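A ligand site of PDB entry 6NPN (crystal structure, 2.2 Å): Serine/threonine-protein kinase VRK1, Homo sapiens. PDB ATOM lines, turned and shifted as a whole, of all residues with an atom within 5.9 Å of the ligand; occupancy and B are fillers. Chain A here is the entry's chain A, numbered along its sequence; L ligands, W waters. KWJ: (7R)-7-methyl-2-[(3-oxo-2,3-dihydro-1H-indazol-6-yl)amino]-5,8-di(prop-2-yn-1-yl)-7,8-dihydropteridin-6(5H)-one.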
ATOM      1  N   ILE A  43      15.033 -30.387 -27.299  1.00  0.00           N
ATOM      2  CA  ILE A  43      16.409 -30.715 -27.575  1.00  0.00           C
ATOM      3  C   ILE A  43      16.761 -32.007 -26.836  1.00  0.00           C
ATOM      4  O   ILE A  43      16.926 -33.023 -27.461  1.00  0.00           O
ATOM      5  CB  ILE A  43      17.262 -29.544 -27.067  1.00  0.00           C
ATOM      6  CG1 ILE A  43      16.857 -28.241 -27.768  1.00  0.00           C
ATOM      7  CG2 ILE A  43      18.751 -29.860 -27.167  1.00  0.00           C
ATOM      8  CD1 ILE A  43      17.358 -27.006 -27.062  1.00  0.00           C
ATOM      9  N   PHE A  48      21.187 -32.280 -22.954  1.00  0.00           N
ATOM     10  CA  PHE A  48      20.650 -33.262 -22.002  1.00  0.00           C
ATOM     11  C   PHE A  48      19.773 -32.612 -20.934  1.00  0.00           C
ATOM     12  O   PHE A  48      20.083 -31.495 -20.460  1.00  0.00           O
ATOM     13  N   ILE A  51      14.674 -29.589 -21.845  1.00  0.00           N
ATOM     14  CA  ILE A  51      15.078 -28.307 -22.442  1.00  0.00           C
ATOM     15  C   ILE A  51      14.436 -28.207 -23.826  1.00  0.00           C
ATOM     16  O   ILE A  51      14.470 -29.165 -24.604  1.00  0.00           O
ATOM     17  CB  ILE A  51      16.609 -28.187 -22.523  1.00  0.00           C
ATOM     18  CG1 ILE A  51      17.260 -28.353 -21.145  1.00  0.00           C
ATOM     19  CG2 ILE A  51      17.007 -26.863 -23.179  1.00  0.00           C
ATOM     20  CD1 ILE A  51      18.759 -28.089 -21.087  1.00  0.00           C
ATOM     21  N   LEU A  53      13.851 -25.321 -27.339  1.00  0.00           N
ATOM     22  CA  LEU A  53      14.064 -24.039 -27.972  1.00  0.00           C
ATOM     23  C   LEU A  53      12.932 -23.100 -27.507  1.00  0.00           C
ATOM     24  O   LEU A  53      11.871 -23.526 -27.095  1.00  0.00           O
ATOM     25  CB  LEU A  53      14.030 -24.210 -29.500  1.00  0.00           C
ATOM     26  CG  LEU A  53      15.147 -25.027 -30.135  1.00  0.00           C
ATOM     27  CD1 LEU A  53      14.920 -25.111 -31.648  1.00  0.00           C
ATOM     28  CD2 LEU A  53      16.531 -24.447 -29.855  1.00  0.00           C
ATOM     29  N   SER A  64      13.960 -23.201 -35.918  1.00  0.00           N
ATOM     30  CA  SER A  64      15.094 -24.071 -35.572  1.00  0.00           C
ATOM     31  C   SER A  64      16.329 -23.209 -35.243  1.00  0.00           C
ATOM     32  O   SER A  64      17.289 -23.715 -34.682  1.00  0.00           O
ATOM     33  CB  SER A  64      15.353 -25.063 -36.682  1.00  0.00           C
ATOM     34  OG  SER A  64      16.074 -24.447 -37.750  1.00  0.00           O
ATOM     35  N   VAL A  69      16.571 -20.934 -25.074  1.00  0.00           N
ATOM     36  CA  VAL A  69      16.075 -22.208 -24.646  1.00  0.00           C
ATOM     37  C   VAL A  69      15.347 -21.977 -23.331  1.00  0.00           C
ATOM     38  O   VAL A  69      15.593 -20.985 -22.660  1.00  0.00           O
ATOM     39  CB  VAL A  69      17.199 -23.233 -24.448  1.00  0.00           C
ATOM     40  CG1 VAL A  69      18.000 -23.417 -25.732  1.00  0.00           C
ATOM     41  CG2 VAL A  69      18.099 -22.858 -23.270  1.00  0.00           C
ATOM     42  N   LYS A  71      14.538 -24.207 -19.826  1.00  0.00           N
ATOM     43  CA  LYS A  71      14.871 -25.353 -19.033  1.00  0.00           C
ATOM     44  C   LYS A  71      13.780 -25.499 -17.973  1.00  0.00           C
ATOM     45  O   LYS A  71      13.411 -24.527 -17.348  1.00  0.00           O
ATOM     46  CB  LYS A  71      16.260 -25.145 -18.433  1.00  0.00           C
ATOM     47  CG  LYS A  71      16.842 -26.305 -17.651  1.00  0.00           C
ATOM     48  CD  LYS A  71      18.365 -26.248 -17.574  1.00  0.00           C
ATOM     49  CE  LYS A  71      18.961 -27.413 -16.817  1.00  0.00           C
ATOM     50  NZ  LYS A  71      20.386 -27.149 -16.510  1.00  0.00           N
ATOM     51  N   GLU A  83      20.625 -23.348  -9.693  1.00  0.00           N
ATOM     52  CA  GLU A  83      21.008 -22.783 -10.972  1.00  0.00           C
ATOM     53  C   GLU A  83      20.344 -21.428 -11.178  1.00  0.00           C
ATOM     54  O   GLU A  83      20.983 -20.478 -11.603  1.00  0.00           O
ATOM     55  CB  GLU A  83      20.632 -23.764 -12.077  1.00  0.00           C
ATOM     56  CG  GLU A  83      21.132 -23.337 -13.427  1.00  0.00           C
ATOM     57  CD  GLU A  83      21.216 -24.468 -14.434  1.00  0.00           C
ATOM     58  OE1 GLU A  83      20.273 -25.315 -14.487  1.00  0.00           O
ATOM     59  OE2 GLU A  83      22.246 -24.533 -15.150  1.00  0.00           O
ATOM     60  N   TYR A  87      21.957 -17.696 -11.809  1.00  0.00           N
ATOM     61  CA  TYR A  87      21.678 -16.889 -12.992  1.00  0.00           C
ATOM     62  C   TYR A  87      21.132 -15.516 -12.567  1.00  0.00           C
ATOM     63  O   TYR A  87      21.528 -14.498 -13.105  1.00  0.00           O
ATOM     64  CB  TYR A  87      20.743 -17.633 -13.954  1.00  0.00           C
ATOM     65  CG  TYR A  87      21.485 -18.564 -14.880  1.00  0.00           C
ATOM     66  CD1 TYR A  87      22.219 -18.042 -15.933  1.00  0.00           C
ATOM     67  CD2 TYR A  87      21.436 -19.943 -14.763  1.00  0.00           C
ATOM     68  CE1 TYR A  87      22.927 -18.855 -16.808  1.00  0.00           C
ATOM     69  CE2 TYR A  87      22.120 -20.761 -15.638  1.00  0.00           C
ATOM     70  CZ  TYR A  87      22.883 -20.222 -16.656  1.00  0.00           C
ATOM     71  OH  TYR A  87      23.552 -21.005 -17.546  1.00  0.00           O
ATOM     72  N   PRO A 111      26.324 -17.692 -19.854  1.00  0.00           N
ATOM     73  CA  PRO A 111      25.015 -17.535 -20.505  1.00  0.00           C
ATOM     74  C   PRO A 111      24.162 -16.484 -19.792  1.00  0.00           C
ATOM     75  O   PRO A 111      24.215 -16.342 -18.561  1.00  0.00           O
ATOM     76  CB  PRO A 111      24.356 -18.903 -20.368  1.00  0.00           C
ATOM     77  CG  PRO A 111      25.507 -19.851 -20.055  1.00  0.00           C
ATOM     78  CD  PRO A 111      26.483 -19.018 -19.250  1.00  0.00           C
ATOM     79  N   MET A 131      17.164 -19.098 -21.038  1.00  0.00           N
ATOM     80  CA  MET A 131      18.559 -18.794 -21.242  1.00  0.00           C
ATOM     81  C   MET A 131      18.887 -18.674 -22.720  1.00  0.00           C
ATOM     82  O   MET A 131      18.048 -19.016 -23.557  1.00  0.00           O
ATOM     83  CB  MET A 131      19.413 -19.890 -20.623  1.00  0.00           C
ATOM     84  CG  MET A 131      19.411 -19.723 -19.103  1.00  0.00           C
ATOM     85  SD  MET A 131      19.895 -21.217 -18.263  1.00  0.00           S
ATOM     86  CE  MET A 131      18.661 -22.336 -18.899  1.00  0.00           C
ATOM     87  N   ASP A 132      20.107 -18.166 -22.991  1.00  0.00           N
ATOM     88  CA  ASP A 132      20.711 -18.148 -24.318  1.00  0.00           C
ATOM     89  C   ASP A 132      20.691 -19.552 -24.935  1.00  0.00           C
ATOM     90  O   ASP A 132      20.898 -20.548 -24.241  1.00  0.00           O
ATOM     91  CB  ASP A 132      22.173 -17.695 -24.272  1.00  0.00           C
ATOM     92  CG  ASP A 132      22.392 -16.216 -24.048  1.00  0.00           C
ATOM     93  OD1 ASP A 132      21.513 -15.453 -24.452  1.00  0.00           O
ATOM     94  OD2 ASP A 132      23.472 -15.823 -23.539  1.00  0.00           O
ATOM     95  N   ARG A 133      20.389 -19.607 -26.239  1.00  0.00           N
ATOM     96  CA  ARG A 133      20.531 -20.816 -27.036  1.00  0.00           C
ATOM     97  C   ARG A 133      21.944 -20.850 -27.651  1.00  0.00           C
ATOM     98  O   ARG A 133      22.438 -19.848 -28.178  1.00  0.00           O
ATOM     99  CB  ARG A 133      19.509 -20.877 -28.168  1.00  0.00           C
ATOM    100  CG  ARG A 133      19.652 -22.063 -29.109  1.00  0.00           C
ATOM    101  CD  ARG A 133      20.471 -21.729 -30.368  1.00  0.00           C
ATOM    102  NE  ARG A 133      20.598 -22.890 -31.252  1.00  0.00           N
ATOM    103  CZ  ARG A 133      19.710 -23.244 -32.160  1.00  0.00           C
ATOM    104  NH1 ARG A 133      19.795 -24.426 -32.750  1.00  0.00           N
ATOM    105  NH2 ARG A 133      18.717 -22.442 -32.473  1.00  0.00           N
ATOM    106  N   PHE A 134      22.573 -22.023 -27.605  1.00  0.00           N
ATOM    107  CA  PHE A 134      23.930 -22.197 -28.130  1.00  0.00           C
ATOM    108  C   PHE A 134      23.932 -23.229 -29.260  1.00  0.00           C
ATOM    109  O   PHE A 134      22.906 -23.828 -29.558  1.00  0.00           O
ATOM    110  CB  PHE A 134      24.854 -22.632 -26.977  1.00  0.00           C
ATOM    111  CG  PHE A 134      24.995 -21.574 -25.913  1.00  0.00           C
ATOM    112  CD1 PHE A 134      25.648 -20.383 -26.192  1.00  0.00           C
ATOM    113  CD2 PHE A 134      24.399 -21.728 -24.681  1.00  0.00           C
ATOM    114  CE1 PHE A 134      25.683 -19.380 -25.246  1.00  0.00           C
ATOM    115  CE2 PHE A 134      24.504 -20.745 -23.716  1.00  0.00           C
ATOM    116  CZ  PHE A 134      25.131 -19.572 -23.994  1.00  0.00           C
ATOM    117  N   GLY A 135      25.110 -23.430 -29.856  1.00  0.00           N
ATOM    118  CA  GLY A 135      25.390 -24.493 -30.790  1.00  0.00           C
ATOM    119  C   GLY A 135      25.832 -25.772 -30.096  1.00  0.00           C
ATOM    120  O   GLY A 135      25.286 -26.162 -29.081  1.00  0.00           O
ATOM    121  N   SER A 136      26.822 -26.432 -30.683  1.00  0.00           N
ATOM    122  CA  SER A 136      27.298 -27.724 -30.212  1.00  0.00           C
ATOM    123  C   SER A 136      28.079 -27.589 -28.890  1.00  0.00           C
ATOM    124  O   SER A 136      28.758 -26.578 -28.632  1.00  0.00           O
ATOM    125  CB  SER A 136      28.142 -28.351 -31.291  1.00  0.00           C
ATOM    126  OG  SER A 136      28.581 -29.649 -30.897  1.00  0.00           O
ATOM    127  N   ASP A 137      28.013 -28.656 -28.090  1.00  0.00           N
ATOM    128  CA  ASP A 137      28.929 -28.873 -26.984  1.00  0.00           C
ATOM    129  C   ASP A 137      30.308 -29.302 -27.517  1.00  0.00           C
ATOM    130  O   ASP A 137      30.427 -29.812 -28.626  1.00  0.00           O
ATOM    131  CB  ASP A 137      28.349 -29.896 -26.002  1.00  0.00           C
ATOM    132  CG  ASP A 137      28.330 -31.322 -26.520  1.00  0.00           C
ATOM    133  OD1 ASP A 137      27.369 -31.651 -27.254  1.00  0.00           O
ATOM    134  OD2 ASP A 137      29.270 -32.064 -26.225  1.00  0.00           O
ATOM    135  N   SER A 181      31.645 -31.354 -22.059  1.00  0.00           N
ATOM    136  CA  SER A 181      30.179 -31.450 -22.225  1.00  0.00           C
ATOM    137  C   SER A 181      29.435 -30.238 -21.611  1.00  0.00           C
ATOM    138  O   SER A 181      28.249 -30.025 -21.915  1.00  0.00           O
ATOM    139  CB  SER A 181      29.632 -32.767 -21.735  1.00  0.00           C
ATOM    140  OG  SER A 181      29.745 -32.914 -20.321  1.00  0.00           O
ATOM    141  N   ASN A 182      30.112 -29.410 -20.808  1.00  0.00           N
ATOM    142  CA  ASN A 182      29.492 -28.220 -20.203  1.00  0.00           C
ATOM    143  C   ASN A 182      30.019 -26.957 -20.891  1.00  0.00           C
ATOM    144  O   ASN A 182      29.845 -25.857 -20.391  1.00  0.00           O
ATOM    145  CB  ASN A 182      29.718 -28.150 -18.689  1.00  0.00           C
ATOM    146  CG  ASN A 182      28.879 -29.135 -17.892  1.00  0.00           C
ATOM    147  OD1 ASN A 182      27.788 -29.487 -18.322  1.00  0.00           O
ATOM    148  ND2 ASN A 182      29.367 -29.581 -16.745  1.00  0.00           N
ATOM    149  N   LEU A 184      29.781 -24.952 -24.490  1.00  0.00           N
ATOM    150  CA  LEU A 184      28.993 -24.874 -25.730  1.00  0.00           C
ATOM    151  C   LEU A 184      29.478 -23.673 -26.534  1.00  0.00           C
ATOM    152  O   LEU A 184      29.858 -22.631 -25.971  1.00  0.00           O
ATOM    153  CB  LEU A 184      27.489 -24.702 -25.436  1.00  0.00           C
ATOM    154  CG  LEU A 184      26.805 -25.602 -24.420  1.00  0.00           C
ATOM    155  CD1 LEU A 184      25.293 -25.436 -24.489  1.00  0.00           C
ATOM    156  CD2 LEU A 184      27.177 -27.041 -24.580  1.00  0.00           C
ATOM    157  N   VAL A 196      28.223 -23.770 -19.207  1.00  0.00           N
ATOM    158  CA  VAL A 196      26.854 -23.984 -18.797  1.00  0.00           C
ATOM    159  C   VAL A 196      26.783 -24.977 -17.621  1.00  0.00           C
ATOM    160  O   VAL A 196      27.805 -25.542 -17.187  1.00  0.00           O
ATOM    161  CB  VAL A 196      25.977 -24.461 -19.965  1.00  0.00           C
ATOM    162  CG1 VAL A 196      26.052 -23.489 -21.136  1.00  0.00           C
ATOM    163  CG2 VAL A 196      26.328 -25.874 -20.420  1.00  0.00           C
ATOM    164  N   ASP A 197      25.564 -25.110 -17.085  1.00  0.00           N
ATOM    165  CA  ASP A 197      25.164 -26.071 -16.086  1.00  0.00           C
ATOM    166  C   ASP A 197      25.704 -25.651 -14.710  1.00  0.00           C
ATOM    167  O   ASP A 197      26.782 -26.056 -14.312  1.00  0.00           O
ATOM    168  CB  ASP A 197      25.560 -27.501 -16.420  1.00  0.00           C
ATOM    169  CG  ASP A 197      24.837 -28.522 -15.529  1.00  0.00           C
ATOM    170  OD1 ASP A 197      24.346 -28.131 -14.427  1.00  0.00           O
ATOM    171  OD2 ASP A 197      24.773 -29.696 -15.924  1.00  0.00           O
ATOM    172  N   TYR A 198      24.897 -24.842 -13.993  1.00  0.00           N
ATOM    173  CA  TYR A 198      25.235 -24.334 -12.701  1.00  0.00           C
ATOM    174  C   TYR A 198      24.393 -25.030 -11.638  1.00  0.00           C
ATOM    175  O   TYR A 198      24.280 -24.527 -10.524  1.00  0.00           O
ATOM    176  CB  TYR A 198      25.078 -22.798 -12.673  1.00  0.00           C
ATOM    177  CG  TYR A 198      26.048 -22.119 -13.604  1.00  0.00           C
ATOM    178  CD1 TYR A 198      25.771 -21.974 -14.956  1.00  0.00           C
ATOM    179  CD2 TYR A 198      27.297 -21.724 -13.164  1.00  0.00           C
ATOM    180  CE1 TYR A 198      26.697 -21.418 -15.829  1.00  0.00           C
ATOM    181  CE2 TYR A 198      28.220 -21.158 -14.018  1.00  0.00           C
ATOM    182  CZ  TYR A 198      27.937 -21.026 -15.360  1.00  0.00           C
ATOM    183  OH  TYR A 198      28.858 -20.436 -16.195  1.00  0.00           O
HETATM  184  C4  KWJ L   1      22.292 -28.645 -27.697  1.00  0.00           C
HETATM  185  C14 KWJ L   1      22.277 -22.631 -20.540  1.00  0.00           C
HETATM  186  C5  KWJ L   1      22.527 -29.060 -26.256  1.00  0.00           C
HETATM  187  C6  KWJ L   1      23.996 -29.310 -25.997  1.00  0.00           C
HETATM  188  C11 KWJ L   1      21.618 -24.605 -24.946  1.00  0.00           C
HETATM  189  C7  KWJ L   1      21.685 -28.579 -23.941  1.00  0.00           C
HETATM  190  C8  KWJ L   1      22.851 -28.511 -23.066  1.00  0.00           C
HETATM  191  C9  KWJ L   1      23.806 -28.438 -22.378  1.00  0.00           C
HETATM  192  C10 KWJ L   1      21.881 -26.769 -25.603  1.00  0.00           C
HETATM  193  C12 KWJ L   1      21.721 -23.799 -22.566  1.00  0.00           C
HETATM  194  C13 KWJ L   1      22.003 -22.615 -21.878  1.00  0.00           C
HETATM  195  N1  KWJ L   1      22.085 -27.319 -27.968  1.00  0.00           N
HETATM  196  N2  KWJ L   1      22.011 -28.095 -25.282  1.00  0.00           N
HETATM  197  C3  KWJ L   1      22.042 -26.896 -29.362  1.00  0.00           C
HETATM  198  N3  KWJ L   1      21.731 -25.891 -24.607  1.00  0.00           N
HETATM  199  C1  KWJ L   1      19.589 -26.673 -30.311  1.00  0.00           C
HETATM  200  C2  KWJ L   1      20.681 -26.789 -29.893  1.00  0.00           C
HETATM  201  O1  KWJ L   1      22.277 -29.484 -28.584  1.00  0.00           O
HETATM  202  N4  KWJ L   1      21.459 -23.704 -23.947  1.00  0.00           N
HETATM  203  C15 KWJ L   1      22.269 -23.844 -19.865  1.00  0.00           C
HETATM  204  C16 KWJ L   1      22.495 -24.219 -18.507  1.00  0.00           C
HETATM  205  O2  KWJ L   1      22.777 -23.500 -17.553  1.00  0.00           O
HETATM  206  N5  KWJ L   1      22.343 -25.554 -18.420  1.00  0.00           N
HETATM  207  N6  KWJ L   1      22.040 -26.059 -19.660  1.00  0.00           N
HETATM  208  C17 KWJ L   1      21.974 -25.028 -20.560  1.00  0.00           C
HETATM  209  C18 KWJ L   1      21.702 -25.030 -21.928  1.00  0.00           C
HETATM  210  N7  KWJ L   1      21.643 -24.127 -26.197  1.00  0.00           N
HETATM  211  C19 KWJ L   1      21.795 -24.997 -27.183  1.00  0.00           C
HETATM  212  C20 KWJ L   1      21.923 -26.364 -26.947  1.00  0.00           C
HETATM  213  O   HOH W   1      21.999 -28.841 -19.355  1.00  0.00           O
HETATM  214  O   HOH W   2      22.393 -25.679 -32.493  1.00  0.00           O
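O2 of the ligand sits at hydrogen-bond distance from OH of Tyr 87. The side-chain carboxylate (OE2) of Glu 83 lies close to a nitrogen (N5) of the ligand (3.4 Å). The backbone NH (N) of Phe 134 is in hydrogen-bond range of a nitrogen (N7) of the ligand. The backbone carbonyl oxygen (O) of Asp 132 sits at hydrogen-bond distance from a nitrogen (N4) of the ligand. The backbone NH (N) of Asp 197 lies within hydrogen-bond range of an oxygen (O2) of the ligand, at 3.3 Å.
The side-chain sulfur of Met 131 sits close to the side-chain hydroxyl of Tyr 87 (3.7 Å). The side-chain carboxylate (OE1) of Glu 83 lies within salt-bridge range of the side-chain amino group (NZ) of Lys 71, 2.7 Å away. N of Tyr 198 lies within hydrogen-bond range of OE2 of Glu 83 (2.9 Å). The guanidinium group (NH2) of Arg 133 lies within hydrogen-bond range of the backbone carbonyl oxygen (O) of Ser 64, at 2.9 Å. O of Met 131 is in hydrogen-bond range of N of Val 69 (2.9 Å). The backbone NH of Val 196 lies within hydrogen-bond range of the backbone carbonyl oxygen of Asn 182 (2.9 Å). The backbone carbonyl oxygen (O) of Ile 51 is in hydrogen-bond range of the backbone NH (N) of Ile 43, 3.0 Å away.
The side-chain amino group (NZ) of Lys 71 sits close to a nitrogen (N5) of the ligand (3.2 Å). SD of Met 131 sits close to O2 of the ligand (3.7 Å). Residues that only touch the ligand: Ile 43, Phe 48, Leu 53, Val 69, Arg 133, Gly 135, Leu 184 and Val 196. Hydrophobic or aromatic side chains within 4 Å of the ligand: Ile 43, Leu 53, Val 69, Tyr 87, Met 131, Phe 134, Leu 184 and Val 196. 15 residues have an atom within 4 Å of the ligand: Ile 43, Phe 48, Leu 53, Val 69, Lys 71, Glu 83, Tyr 87, Met 131, Asp 132, Arg 133, Phe 134, Gly 135, Leu 184, Val 196 and Asp 197. The nearest printed residue that does not touch the ligand is Ile 51 (4.1 Å).
Water W1 bridges N6 of the ligand (2.8 Å) and O of Phe 48 (3.5 Å).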
